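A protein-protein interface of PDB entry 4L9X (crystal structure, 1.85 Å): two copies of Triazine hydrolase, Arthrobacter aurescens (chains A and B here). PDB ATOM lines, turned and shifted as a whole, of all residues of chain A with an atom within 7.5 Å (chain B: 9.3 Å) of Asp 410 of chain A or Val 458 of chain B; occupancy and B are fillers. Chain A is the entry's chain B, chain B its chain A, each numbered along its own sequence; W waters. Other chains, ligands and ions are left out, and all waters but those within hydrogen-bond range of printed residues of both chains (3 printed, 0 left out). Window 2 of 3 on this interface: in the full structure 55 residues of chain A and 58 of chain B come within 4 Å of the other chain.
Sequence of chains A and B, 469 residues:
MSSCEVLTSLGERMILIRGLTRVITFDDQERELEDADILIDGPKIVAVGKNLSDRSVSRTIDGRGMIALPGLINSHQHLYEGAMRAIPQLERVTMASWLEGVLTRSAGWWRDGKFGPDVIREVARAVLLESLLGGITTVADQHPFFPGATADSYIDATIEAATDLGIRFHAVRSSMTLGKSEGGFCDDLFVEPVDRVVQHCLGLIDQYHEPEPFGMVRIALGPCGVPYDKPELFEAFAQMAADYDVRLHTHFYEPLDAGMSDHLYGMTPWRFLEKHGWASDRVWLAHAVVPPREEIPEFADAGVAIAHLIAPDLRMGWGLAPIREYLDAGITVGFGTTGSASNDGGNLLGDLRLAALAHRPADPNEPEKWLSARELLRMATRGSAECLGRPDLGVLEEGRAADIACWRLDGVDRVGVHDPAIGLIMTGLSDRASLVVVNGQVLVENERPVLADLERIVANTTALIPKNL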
ATOM      1  N   ARG A  64     -31.114 -20.589  -8.597  1.00  0.00           N
ATOM      2  CA  ARG A  64     -31.457 -21.173  -9.885  1.00  0.00           C
ATOM      3  C   ARG A  64     -30.184 -21.555 -10.643  1.00  0.00           C
ATOM      4  O   ARG A  64     -29.213 -20.799 -10.672  1.00  0.00           O
ATOM      5  CB  ARG A  64     -32.364 -20.248 -10.712  1.00  0.00           C
ATOM      6  CG  ARG A  64     -33.800 -20.158 -10.171  1.00  0.00           C
ATOM      7  CD  ARG A  64     -34.617 -19.143 -10.958  1.00  0.00           C
ATOM      8  NE  ARG A  64     -34.010 -17.818 -10.897  1.00  0.00           N
ATOM      9  CZ  ARG A  64     -34.335 -16.805 -11.696  1.00  0.00           C
ATOM     10  NH1 ARG A  64     -35.254 -16.966 -12.640  1.00  0.00           N
ATOM     11  NH2 ARG A  64     -33.726 -15.635 -11.561  1.00  0.00           N
ATOM     12  N   GLY A  65     -30.190 -22.758 -11.215  1.00  0.00           N
ATOM     13  CA  GLY A  65     -29.069 -23.233 -12.006  1.00  0.00           C
ATOM     14  C   GLY A  65     -27.936 -23.819 -11.178  1.00  0.00           C
ATOM     15  O   GLY A  65     -26.866 -24.098 -11.727  1.00  0.00           O
ATOM     16  N   MET A  66     -28.163 -24.023  -9.870  1.00  0.00           N
ATOM     17  CA  MET A  66     -27.120 -24.594  -8.997  1.00  0.00           C
ATOM     18  C   MET A  66     -27.543 -25.921  -8.388  1.00  0.00           C
ATOM     19  O   MET A  66     -28.732 -26.172  -8.207  1.00  0.00           O
ATOM     20  CB  MET A  66     -26.782 -23.638  -7.852  1.00  0.00           C
ATOM     21  CG  MET A  66     -26.275 -22.280  -8.281  1.00  0.00           C
ATOM     22  SD  MET A  66     -25.599 -21.389  -6.863  1.00  0.00           S
ATOM     23  CE  MET A  66     -25.370 -19.758  -7.581  1.00  0.00           C
ATOM     24  N   TRP A 407     -22.719 -25.558  -6.594  1.00  0.00           N
ATOM     25  CA  TRP A 407     -22.010 -25.413  -7.867  1.00  0.00           C
ATOM     26  C   TRP A 407     -23.026 -25.110  -8.966  1.00  0.00           C
ATOM     27  O   TRP A 407     -24.114 -25.696  -8.998  1.00  0.00           O
ATOM     28  CB  TRP A 407     -21.288 -26.714  -8.234  1.00  0.00           C
ATOM     29  CG  TRP A 407     -20.045 -26.991  -7.428  1.00  0.00           C
ATOM     30  CD1 TRP A 407     -18.752 -26.760  -7.819  1.00  0.00           C
ATOM     31  CD2 TRP A 407     -19.972 -27.568  -6.110  1.00  0.00           C
ATOM     32  NE1 TRP A 407     -17.879 -27.161  -6.825  1.00  0.00           N
ATOM     33  CE2 TRP A 407     -18.602 -27.665  -5.769  1.00  0.00           C
ATOM     34  CE3 TRP A 407     -20.928 -28.031  -5.195  1.00  0.00           C
ATOM     35  CZ2 TRP A 407     -18.161 -28.188  -4.542  1.00  0.00           C
ATOM     36  CZ3 TRP A 407     -20.494 -28.554  -3.972  1.00  0.00           C
ATOM     37  CH2 TRP A 407     -19.114 -28.626  -3.659  1.00  0.00           C
ATOM     38  N   ARG A 408     -22.671 -24.193  -9.860  1.00  0.00           N
ATOM     39  CA  ARG A 408     -23.518 -23.894 -11.010  1.00  0.00           C
ATOM     40  C   ARG A 408     -23.513 -25.059 -11.980  1.00  0.00           C
ATOM     41  O   ARG A 408     -22.492 -25.749 -12.141  1.00  0.00           O
ATOM     42  CB  ARG A 408     -23.026 -22.634 -11.717  1.00  0.00           C
ATOM     43  CG  ARG A 408     -23.125 -21.378 -10.868  1.00  0.00           C
ATOM     44  CD  ARG A 408     -23.308 -20.159 -11.767  1.00  0.00           C
ATOM     45  NE  ARG A 408     -24.585 -20.252 -12.472  1.00  0.00           N
ATOM     46  CZ  ARG A 408     -25.735 -19.782 -11.989  1.00  0.00           C
ATOM     47  NH1 ARG A 408     -25.756 -19.178 -10.808  1.00  0.00           N
ATOM     48  NH2 ARG A 408     -26.862 -19.910 -12.683  1.00  0.00           N
ATOM     49  N   LEU A 409     -24.653 -25.271 -12.628  1.00  0.00           N
ATOM     50  CA  LEU A 409     -24.808 -26.355 -13.584  1.00  0.00           C
ATOM     51  C   LEU A 409     -24.884 -25.846 -15.022  1.00  0.00           C
ATOM     52  O   LEU A 409     -25.040 -26.641 -15.939  1.00  0.00           O
ATOM     53  CB  LEU A 409     -26.083 -27.148 -13.271  1.00  0.00           C
ATOM     54  CG  LEU A 409     -26.101 -27.825 -11.900  1.00  0.00           C
ATOM     55  CD1 LEU A 409     -27.521 -28.253 -11.525  1.00  0.00           C
ATOM     56  CD2 LEU A 409     -25.127 -29.012 -11.851  1.00  0.00           C
ATOM     57  N   ASP A 410     -24.778 -24.535 -15.213  1.00  0.00           N
ATOM     58  CA  ASP A 410     -25.073 -23.935 -16.513  1.00  0.00           C
ATOM     59  C   ASP A 410     -23.846 -23.502 -17.311  1.00  0.00           C
ATOM     60  O   ASP A 410     -23.936 -22.637 -18.198  1.00  0.00           O
ATOM     61  CB  ASP A 410     -26.070 -22.764 -16.361  1.00  0.00           C
ATOM     62  CG  ASP A 410     -25.565 -21.664 -15.426  1.00  0.00           C
ATOM     63  OD1 ASP A 410     -24.450 -21.800 -14.863  1.00  0.00           O
ATOM     64  OD2 ASP A 410     -26.297 -20.662 -15.247  1.00  0.00           O
ATOM     65  N   GLY A 411     -22.703 -24.116 -17.011  1.00  0.00           N
ATOM     66  CA  GLY A 411     -21.475 -23.811 -17.716  1.00  0.00           C
ATOM     67  C   GLY A 411     -21.430 -24.576 -19.020  1.00  0.00           C
ATOM     68  O   GLY A 411     -22.109 -25.601 -19.177  1.00  0.00           O
ATOM     69  N   VAL A 412     -20.640 -24.082 -19.965  1.00  0.00           N
ATOM     70  CA  VAL A 412     -20.575 -24.732 -21.260  1.00  0.00           C
ATOM     71  C   VAL A 412     -20.004 -26.148 -21.120  1.00  0.00           C
ATOM     72  O   VAL A 412     -20.310 -27.023 -21.932  1.00  0.00           O
ATOM     73  CB  VAL A 412     -19.735 -23.945 -22.264  1.00  0.00           C
ATOM     74  CG1 VAL A 412     -18.237 -23.992 -21.872  1.00  0.00           C
ATOM     75  CG2 VAL A 412     -19.963 -24.505 -23.664  1.00  0.00           C
ATOM     76  N   ASP A 413     -19.187 -26.359 -20.089  1.00  0.00           N
ATOM     77  CA  ASP A 413     -18.576 -27.668 -19.835  1.00  0.00           C
ATOM     78  C   ASP A 413     -19.506 -28.675 -19.118  1.00  0.00           C
ATOM     79  O   ASP A 413     -19.102 -29.810 -18.852  1.00  0.00           O
ATOM     80  CB  ASP A 413     -17.267 -27.514 -19.054  1.00  0.00           C
ATOM     81  CG  ASP A 413     -17.421 -26.661 -17.790  1.00  0.00           C
ATOM     82  OD1 ASP A 413     -18.397 -25.879 -17.687  1.00  0.00           O
ATOM     83  OD2 ASP A 413     -16.543 -26.755 -16.904  1.00  0.00           O
ATOM     84  N   ARG A 414     -20.737 -28.271 -18.811  1.00  0.00           N
ATOM     85  CA  ARG A 414     -21.710 -29.202 -18.230  1.00  0.00           C
ATOM     86  C   ARG A 414     -22.989 -29.332 -19.050  1.00  0.00           C
ATOM     87  O   ARG A 414     -23.990 -29.888 -18.578  1.00  0.00           O
ATOM     88  CB  ARG A 414     -22.038 -28.838 -16.769  1.00  0.00           C
ATOM     89  CG  ARG A 414     -20.808 -28.735 -15.853  1.00  0.00           C
ATOM     90  CD  ARG A 414     -21.249 -28.704 -14.414  1.00  0.00           C
ATOM     91  NE  ARG A 414     -20.226 -28.256 -13.473  1.00  0.00           N
ATOM     92  CZ  ARG A 414     -19.272 -29.030 -12.958  1.00  0.00           C
ATOM     93  NH1 ARG A 414     -19.169 -30.311 -13.315  1.00  0.00           N
ATOM     94  NH2 ARG A 414     -18.424 -28.513 -12.073  1.00  0.00           N
ATOM     95  N   VAL A 415     -22.955 -28.843 -20.285  1.00  0.00           N
ATOM     96  CA  VAL A 415     -24.072 -29.040 -21.207  1.00  0.00           C
ATOM     97  C   VAL A 415     -24.228 -30.540 -21.481  1.00  0.00           C
ATOM     98  O   VAL A 415     -23.238 -31.248 -21.606  1.00  0.00           O
ATOM     99  CB  VAL A 415     -23.818 -28.287 -22.527  1.00  0.00           C
ATOM    100  CG1 VAL A 415     -24.823 -28.698 -23.583  1.00  0.00           C
ATOM    101  CG2 VAL A 415     -23.840 -26.758 -22.299  1.00  0.00           C
ATOM    102  N   GLU B 122     -24.647 -27.976 -32.879  1.00  0.00           N
ATOM    103  CA  GLU B 122     -24.672 -27.183 -31.651  1.00  0.00           C
ATOM    104  C   GLU B 122     -24.038 -27.913 -30.484  1.00  0.00           C
ATOM    105  O   GLU B 122     -23.375 -27.296 -29.655  1.00  0.00           O
ATOM    106  CB  GLU B 122     -26.084 -26.705 -31.320  1.00  0.00           C
ATOM    107  CG  GLU B 122     -26.683 -25.825 -32.435  1.00  0.00           C
ATOM    108  CD  GLU B 122     -25.741 -24.713 -32.900  1.00  0.00           C
ATOM    109  OE1 GLU B 122     -25.103 -24.082 -32.045  1.00  0.00           O
ATOM    110  OE2 GLU B 122     -25.628 -24.475 -34.129  1.00  0.00           O
ATOM    111  N   VAL B 123     -24.225 -29.224 -30.429  1.00  0.00           N
ATOM    112  CA  VAL B 123     -23.503 -30.043 -29.455  1.00  0.00           C
ATOM    113  C   VAL B 123     -21.990 -29.914 -29.688  1.00  0.00           C
ATOM    114  O   VAL B 123     -21.226 -29.737 -28.750  1.00  0.00           O
ATOM    115  CB  VAL B 123     -23.923 -31.519 -29.526  1.00  0.00           C
ATOM    116  CG1 VAL B 123     -22.995 -32.393 -28.658  1.00  0.00           C
ATOM    117  CG2 VAL B 123     -25.379 -31.683 -29.097  1.00  0.00           C
ATOM    118  N   ARG B 125     -20.437 -27.432 -31.179  1.00  0.00           N
ATOM    119  CA  ARG B 125     -20.001 -26.088 -30.818  1.00  0.00           C
ATOM    120  C   ARG B 125     -19.695 -25.991 -29.316  1.00  0.00           C
ATOM    121  O   ARG B 125     -18.688 -25.409 -28.922  1.00  0.00           O
ATOM    122  CB  ARG B 125     -21.047 -25.028 -31.237  1.00  0.00           C
ATOM    123  CG  ARG B 125     -20.477 -23.604 -31.345  1.00  0.00           C
ATOM    124  CD  ARG B 125     -21.587 -22.546 -31.641  1.00  0.00           C
ATOM    125  NE  ARG B 125     -22.479 -22.982 -32.713  1.00  0.00           N
ATOM    126  CZ  ARG B 125     -22.242 -22.799 -34.010  1.00  0.00           C
ATOM    127  NH1 ARG B 125     -21.143 -22.177 -34.409  1.00  0.00           N
ATOM    128  NH2 ARG B 125     -23.108 -23.237 -34.910  1.00  0.00           N
ATOM    129  N   ALA B 126     -20.568 -26.538 -28.479  1.00  0.00           N
ATOM    130  CA  ALA B 126     -20.376 -26.435 -27.029  1.00  0.00           C
ATOM    131  C   ALA B 126     -19.143 -27.213 -26.585  1.00  0.00           C
ATOM    132  O   ALA B 126     -18.333 -26.718 -25.789  1.00  0.00           O
ATOM    133  CB  ALA B 126     -21.607 -26.939 -26.278  1.00  0.00           C
ATOM    134  N   VAL B 127     -19.005 -28.436 -27.082  1.00  0.00           N
ATOM    135  CA  VAL B 127     -17.874 -29.255 -26.652  1.00  0.00           C
ATOM    136  C   VAL B 127     -16.539 -28.684 -27.155  1.00  0.00           C
ATOM    137  O   VAL B 127     -15.546 -28.706 -26.445  1.00  0.00           O
ATOM    138  CB  VAL B 127     -18.036 -30.731 -27.065  1.00  0.00           C
ATOM    139  CG1 VAL B 127     -16.802 -31.521 -26.645  1.00  0.00           C
ATOM    140  CG2 VAL B 127     -19.318 -31.327 -26.425  1.00  0.00           C
ATOM    141  N   LEU B 129     -16.037 -25.471 -27.786  1.00  0.00           N
ATOM    142  CA  LEU B 129     -15.776 -24.281 -26.983  1.00  0.00           C
ATOM    143  C   LEU B 129     -15.222 -24.672 -25.603  1.00  0.00           C
ATOM    144  O   LEU B 129     -14.275 -24.061 -25.107  1.00  0.00           O
ATOM    145  CB  LEU B 129     -17.034 -23.420 -26.828  1.00  0.00           C
ATOM    146  CG  LEU B 129     -16.878 -22.127 -26.020  1.00  0.00           C
ATOM    147  CD1 LEU B 129     -15.702 -21.324 -26.539  1.00  0.00           C
ATOM    148  CD2 LEU B 129     -18.165 -21.279 -26.066  1.00  0.00           C
ATOM    149  N   GLU B 130     -15.792 -25.704 -24.990  1.00  0.00           N
ATOM    150  CA  GLU B 130     -15.203 -26.239 -23.753  1.00  0.00           C
ATOM    151  C   GLU B 130     -13.727 -26.587 -23.996  1.00  0.00           C
ATOM    152  O   GLU B 130     -12.852 -26.336 -23.159  1.00  0.00           O
ATOM    153  CB  GLU B 130     -15.958 -27.494 -23.281  1.00  0.00           C
ATOM    154  CG  GLU B 130     -15.201 -28.290 -22.200  1.00  0.00           C
ATOM    155  CD  GLU B 130     -15.843 -29.639 -21.870  1.00  0.00           C
ATOM    156  OE1 GLU B 130     -16.932 -29.947 -22.404  1.00  0.00           O
ATOM    157  OE2 GLU B 130     -15.241 -30.393 -21.080  1.00  0.00           O
ATOM    158  N   LEU B 133     -11.568 -23.592 -23.991  1.00  0.00           N
ATOM    159  CA  LEU B 133     -11.479 -23.131 -22.613  1.00  0.00           C
ATOM    160  C   LEU B 133     -10.539 -23.967 -21.740  1.00  0.00           C
ATOM    161  O   LEU B 133     -10.037 -23.476 -20.730  1.00  0.00           O
ATOM    162  CB  LEU B 133     -12.863 -23.024 -21.986  1.00  0.00           C
ATOM    163  CG  LEU B 133     -13.732 -21.906 -22.590  1.00  0.00           C
ATOM    164  CD1 LEU B 133     -15.127 -21.947 -21.996  1.00  0.00           C
ATOM    165  CD2 LEU B 133     -13.068 -20.517 -22.387  1.00  0.00           C
ATOM    166  N   ARG B 432      -9.075 -24.340 -16.184  1.00  0.00           N
ATOM    167  CA  ARG B 432      -9.425 -23.320 -17.180  1.00  0.00           C
ATOM    168  C   ARG B 432      -8.169 -22.582 -17.649  1.00  0.00           C
ATOM    169  O   ARG B 432      -7.412 -22.059 -16.834  1.00  0.00           O
ATOM    170  CB  ARG B 432     -10.428 -22.293 -16.598  1.00  0.00           C
ATOM    171  CG  ARG B 432     -11.877 -22.801 -16.422  1.00  0.00           C
ATOM    172  CD  ARG B 432     -12.653 -22.825 -17.745  1.00  0.00           C
ATOM    173  NE  ARG B 432     -13.034 -21.478 -18.182  1.00  0.00           N
ATOM    174  CZ  ARG B 432     -14.235 -20.940 -17.981  1.00  0.00           C
ATOM    175  NH1 ARG B 432     -15.185 -21.646 -17.372  1.00  0.00           N
ATOM    176  NH2 ARG B 432     -14.490 -19.703 -18.400  1.00  0.00           N
ATOM    177  N   ARG B 448     -12.048 -16.447 -20.808  1.00  0.00           N
ATOM    178  CA  ARG B 448     -13.286 -16.232 -21.469  1.00  0.00           C
ATOM    179  C   ARG B 448     -13.148 -16.041 -22.985  1.00  0.00           C
ATOM    180  O   ARG B 448     -12.187 -15.487 -23.407  1.00  0.00           O
ATOM    181  CB  ARG B 448     -14.032 -15.126 -20.736  1.00  0.00           C
ATOM    182  CG  ARG B 448     -14.780 -14.173 -21.579  1.00  0.00           C
ATOM    183  CD  ARG B 448     -16.304 -14.198 -21.471  1.00  0.00           C
ATOM    184  NE  ARG B 448     -16.924 -14.847 -20.341  1.00  0.00           N
ATOM    185  CZ  ARG B 448     -18.241 -14.916 -20.223  1.00  0.00           C
ATOM    186  NH1 ARG B 448     -18.999 -14.408 -21.134  1.00  0.00           N
ATOM    187  NH2 ARG B 448     -18.798 -15.515 -19.224  1.00  0.00           N
ATOM    188  N   PRO B 449     -14.091 -16.575 -23.761  1.00  0.00           N
ATOM    189  CA  PRO B 449     -13.972 -16.507 -25.229  1.00  0.00           C
ATOM    190  C   PRO B 449     -13.970 -15.058 -25.681  1.00  0.00           C
ATOM    191  O   PRO B 449     -14.719 -14.273 -25.108  1.00  0.00           O
ATOM    192  CB  PRO B 449     -15.256 -17.173 -25.726  1.00  0.00           C
ATOM    193  CG  PRO B 449     -15.771 -17.960 -24.565  1.00  0.00           C
ATOM    194  CD  PRO B 449     -15.303 -17.289 -23.325  1.00  0.00           C
ATOM    195  N   ALA B 452     -16.491 -16.026 -29.417  1.00  0.00           N
ATOM    196  CA  ALA B 452     -17.727 -16.779 -29.212  1.00  0.00           C
ATOM    197  C   ALA B 452     -18.544 -16.188 -28.060  1.00  0.00           C
ATOM    198  O   ALA B 452     -17.981 -15.711 -27.075  1.00  0.00           O
ATOM    199  CB  ALA B 452     -17.423 -18.253 -28.944  1.00  0.00           C
ATOM    200  N   ASP B 453     -19.869 -16.229 -28.193  1.00  0.00           N
ATOM    201  CA  ASP B 453     -20.777 -15.795 -27.126  1.00  0.00           C
ATOM    202  C   ASP B 453     -21.111 -16.999 -26.253  1.00  0.00           C
ATOM    203  O   ASP B 453     -21.968 -17.801 -26.593  1.00  0.00           O
ATOM    204  CB  ASP B 453     -22.055 -15.202 -27.734  1.00  0.00           C
ATOM    205  CG  ASP B 453     -23.027 -14.647 -26.682  1.00  0.00           C
ATOM    206  OD1 ASP B 453     -23.112 -15.204 -25.562  1.00  0.00           O
ATOM    207  OD2 ASP B 453     -23.730 -13.659 -26.999  1.00  0.00           O
ATOM    208  N   LEU B 454     -20.414 -17.124 -25.133  1.00  0.00           N
ATOM    209  CA  LEU B 454     -20.542 -18.283 -24.251  1.00  0.00           C
ATOM    210  C   LEU B 454     -21.983 -18.569 -23.782  1.00  0.00           C
ATOM    211  O   LEU B 454     -22.471 -19.705 -23.884  1.00  0.00           O
ATOM    212  CB  LEU B 454     -19.622 -18.098 -23.046  1.00  0.00           C
ATOM    213  CG  LEU B 454     -19.534 -19.209 -22.004  1.00  0.00           C
ATOM    214  CD1 LEU B 454     -19.182 -20.523 -22.675  1.00  0.00           C
ATOM    215  CD2 LEU B 454     -18.490 -18.835 -20.955  1.00  0.00           C
ATOM    216  N   GLU B 455     -22.655 -17.544 -23.263  1.00  0.00           N
ATOM    217  CA  GLU B 455     -23.987 -17.718 -22.684  1.00  0.00           C
ATOM    218  C   GLU B 455     -25.009 -18.131 -23.729  1.00  0.00           C
ATOM    219  O   GLU B 455     -25.862 -18.988 -23.480  1.00  0.00           O
ATOM    220  CB  GLU B 455     -24.454 -16.438 -21.986  1.00  0.00           C
ATOM    221  CG  GLU B 455     -23.812 -16.186 -20.626  1.00  0.00           C
ATOM    222  CD  GLU B 455     -22.442 -15.496 -20.695  1.00  0.00           C
ATOM    223  OE1 GLU B 455     -22.036 -14.981 -21.769  1.00  0.00           O
ATOM    224  OE2 GLU B 455     -21.768 -15.467 -19.647  1.00  0.00           O
ATOM    225  N   ARG B 456     -24.919 -17.521 -24.904  1.00  0.00           N
ATOM    226  CA  ARG B 456     -25.827 -17.840 -25.996  1.00  0.00           C
ATOM    227  C   ARG B 456     -25.644 -19.272 -26.499  1.00  0.00           C
ATOM    228  O   ARG B 456     -26.615 -19.957 -26.795  1.00  0.00           O
ATOM    229  CB  ARG B 456     -25.645 -16.853 -27.154  1.00  0.00           C
ATOM    230  CG  ARG B 456     -26.742 -16.948 -28.205  1.00  0.00           C
ATOM    231  CD  ARG B 456     -26.679 -15.813 -29.244  1.00  0.00           C
ATOM    232  NE  ARG B 456     -27.970 -15.664 -29.930  1.00  0.00           N
ATOM    233  CZ  ARG B 456     -28.326 -16.332 -31.027  1.00  0.00           C
ATOM    234  NH1 ARG B 456     -27.483 -17.190 -31.590  1.00  0.00           N
ATOM    235  NH2 ARG B 456     -29.525 -16.137 -31.564  1.00  0.00           N
ATOM    236  N   ILE B 457     -24.392 -19.709 -26.611  1.00  0.00           N
ATOM    237  CA  ILE B 457     -24.099 -21.079 -27.026  1.00  0.00           C
ATOM    238  C   ILE B 457     -24.640 -22.090 -26.021  1.00  0.00           C
ATOM    239  O   ILE B 457     -25.233 -23.114 -26.401  1.00  0.00           O
ATOM    240  CB  ILE B 457     -22.579 -21.276 -27.240  1.00  0.00           C
ATOM    241  CG1 ILE B 457     -22.130 -20.472 -28.470  1.00  0.00           C
ATOM    242  CG2 ILE B 457     -22.253 -22.765 -27.415  1.00  0.00           C
ATOM    243  CD1 ILE B 457     -20.601 -20.345 -28.646  1.00  0.00           C
ATOM    244  N   VAL B 458     -24.432 -21.818 -24.734  1.00  0.00           N
ATOM    245  CA  VAL B 458     -24.944 -22.716 -23.704  1.00  0.00           C
ATOM    246  C   VAL B 458     -26.467 -22.818 -23.792  1.00  0.00           C
ATOM    247  O   VAL B 458     -27.028 -23.912 -23.750  1.00  0.00           O
ATOM    248  CB  VAL B 458     -24.542 -22.266 -22.289  1.00  0.00           C
ATOM    249  CG1 VAL B 458     -25.315 -23.077 -21.256  1.00  0.00           C
ATOM    250  CG2 VAL B 458     -23.023 -22.425 -22.096  1.00  0.00           C
ATOM    251  N   ALA B 459     -27.136 -21.675 -23.928  1.00  0.00           N
ATOM    252  CA  ALA B 459     -28.595 -21.674 -24.027  1.00  0.00           C
ATOM    253  C   ALA B 459     -29.059 -22.424 -25.270  1.00  0.00           C
ATOM    254  O   ALA B 459     -29.967 -23.253 -25.208  1.00  0.00           O
ATOM    255  CB  ALA B 459     -29.125 -20.235 -24.047  1.00  0.00           C
ATOM    256  N   ASN B 460     -28.436 -22.133 -26.405  1.00  0.00           N
ATOM    257  CA  ASN B 460     -28.870 -22.731 -27.658  1.00  0.00           C
ATOM    258  C   ASN B 460     -28.637 -24.231 -27.674  1.00  0.00           C
ATOM    259  O   ASN B 460     -29.501 -25.008 -28.100  1.00  0.00           O
ATOM    260  CB  ASN B 460     -28.177 -22.070 -28.857  1.00  0.00           C
ATOM    261  CG  ASN B 460     -28.750 -20.692 -29.174  1.00  0.00           C
ATOM    262  OD1 ASN B 460     -29.774 -20.296 -28.616  1.00  0.00           O
ATOM    263  ND2 ASN B 460     -28.099 -19.966 -30.080  1.00  0.00           N
ATOM    264  N   THR B 461     -27.470 -24.646 -27.201  1.00  0.00           N
ATOM    265  CA  THR B 461     -27.167 -26.072 -27.200  1.00  0.00           C
ATOM    266  C   THR B 461     -28.047 -26.838 -26.205  1.00  0.00           C
ATOM    267  O   THR B 461     -28.531 -27.921 -26.512  1.00  0.00           O
ATOM    268  CB  THR B 461     -25.692 -26.329 -26.907  1.00  0.00           C
ATOM    269  OG1 THR B 461     -24.894 -25.671 -27.898  1.00  0.00           O
ATOM    270  CG2 THR B 461     -25.406 -27.818 -26.949  1.00  0.00           C
ATOM    271  N   THR B 462     -28.279 -26.263 -25.028  1.00  0.00           N
ATOM    272  CA  THR B 462     -29.093 -26.927 -24.010  1.00  0.00           C
ATOM    273  C   THR B 462     -30.529 -27.228 -24.481  1.00  0.00           C
ATOM    274  O   THR B 462     -31.086 -28.282 -24.175  1.00  0.00           O
ATOM    275  CB  THR B 462     -29.139 -26.107 -22.700  1.00  0.00           C
ATOM    276  OG1 THR B 462     -27.808 -25.953 -22.180  1.00  0.00           O
ATOM    277  CG2 THR B 462     -30.022 -26.791 -21.662  1.00  0.00           C
ATOM    278  N   ALA B 463     -31.119 -26.299 -25.228  1.00  0.00           N
ATOM    279  CA  ALA B 463     -32.475 -26.473 -25.745  1.00  0.00           C
ATOM    280  C   ALA B 463     -32.564 -27.577 -26.799  1.00  0.00           C
ATOM    281  O   ALA B 463     -33.651 -28.060 -27.099  1.00  0.00           O
ATOM    282  CB  ALA B 463     -33.002 -25.155 -26.312  1.00  0.00           C
ATOM    283  N   LEU B 464     -31.420 -27.999 -27.333  1.00  0.00           N
ATOM    284  CA  LEU B 464     -31.381 -29.008 -28.393  1.00  0.00           C
ATOM    285  C   LEU B 464     -30.965 -30.403 -27.931  1.00  0.00           C
ATOM    286  O   LEU B 464     -31.076 -31.361 -28.692  1.00  0.00           O
ATOM    287  CB  LEU B 464     -30.467 -28.548 -29.538  1.00  0.00           C
ATOM    288  CG  LEU B 464     -30.973 -27.374 -30.376  1.00  0.00           C
ATOM    289  CD1 LEU B 464     -29.842 -26.779 -31.227  1.00  0.00           C
ATOM    290  CD2 LEU B 464     -32.161 -27.786 -31.253  1.00  0.00           C
ATOM    291  N   ILE B 465     -30.482 -30.523 -26.694  1.00  0.00           N
ATOM    292  CA  ILE B 465     -30.150 -31.834 -26.157  1.00  0.00           C
ATOM    293  C   ILE B 465     -31.402 -32.702 -26.174  1.00  0.00           C
ATOM    294  O   ILE B 465     -32.456 -32.276 -25.705  1.00  0.00           O
ATOM    295  CB  ILE B 465     -29.626 -31.757 -24.710  1.00  0.00           C
ATOM    296  CG1 ILE B 465     -28.445 -30.792 -24.614  1.00  0.00           C
ATOM    297  CG2 ILE B 465     -29.210 -33.141 -24.224  1.00  0.00           C
ATOM    298  CD1 ILE B 465     -27.278 -31.216 -25.466  1.00  0.00           C
HETATM  299  O   HOH W   1     -16.997 -31.381 -19.074  1.00  0.00           O
HETATM  300  O   HOH W   2     -19.489 -29.187 -23.414  1.00  0.00           O
HETATM  301  O   HOH W   3     -15.585 -24.116 -15.926  1.00  0.00           O
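Water W1 lies within hydrogen-bond range of O of Asp 413 of chain A and OE2 of Glu 130 of chain B. Water W2 bridges the backbone carbonyl oxygen (O) of Val 412 of chain A and the side-chain carboxylate (OE1) of Glu 130 of chain B. Water W3 bridges NH1 of Arg 432 of chain B (2.9 Å) and OD2 of Asp 413 of chain A (3.0 Å).
No position is printed for both chains. Of the 8 pairs that touch across the chains among the printed residues, none has its exchanged pair printed and touching as well.
The side-chain hydroxyl (OG1) of Thr 461 of chain B lies within hydrogen-bond range of the backbone carbonyl oxygen (O) of Ile 457 of chain B (3.0 Å). The guanidinium group (NH2) of Arg 408 of chain A lies within salt-bridge range of the side-chain carboxylate (OD2) of Asp 410 of chain A (2.7 Å).
Of the 12 printed residues of chain A, 4 touch a printed residue of chain B. Hydrophobic or aromatic side chains of chain A within 4 Å of the printed part of chain B: Val 412 and Val 415. Printed residues of chain B that touch a printed residue of chain A: Ala 126, Glu 130, Leu 133, Leu 454, Val 458, Thr 461 and Ile 465. Hydrophobic or aromatic side chains of chain B that line the printed part of chain A: Ala 126, Leu 133, Leu 454, Val 458 and Ile 465. Among the printed residues, 8 pairs touch across the chains. Among the printed residues, no Asp or Glu carboxylate lies within 4 Å of a Lys or Arg side-chain nitrogen of the other chain.
Asp 410 of chain A touches one residue of chain B. No residue of chain B comes within 4 Å of Gly 411 of chain A. Of the printed residues of chain B, Val 412 of chain A touches Ala 126, Leu 133, Leu 454 and Val 458. Printed residues of chain B within 4 Å of Asp 413 of chain A: Glu 130. Of the printed residues of chain B, Val 415 of chain A touches Thr 461 and Ile 465. Of chain A, only Asp 410 and Val 412 come within 4 Å of Val 458 of chain B. Printed residues of chain A within 4 Å of Ile 465 of chain B: Val 415 (3.99 Å). The nearest residue of chain B that does not touch Asp 410 of chain A is Thr 462 of chain B (6.5 Å). The nearest printed residue of chain A that does not touch Val 458 of chain B is Gly 411 of chain A (4.1 Å). The nearest printed residue of chain A that does not touch Ile 465 of chain B is Arg 414 of chain A (7.6 Å).
Asp 410 of chain A touches Val 458 of chain B. Val 412 of chain A touches Ala 126 of chain B (CG2 to O, 3.5 Å). CG1 of Val 412 of chain A touches CD1 of Leu 133 of chain B, 3.7 Å away. Val 412 of chain A touches Leu 454 of chain B (CB to CD1, 3.5 Å). Asp 413 of chain A touches Glu 130 of chain B (CB to CD, 3.8 Å). CG1 of Val 415 of chain A touches CG2 of Thr 461 of chain B (3.5 Å).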
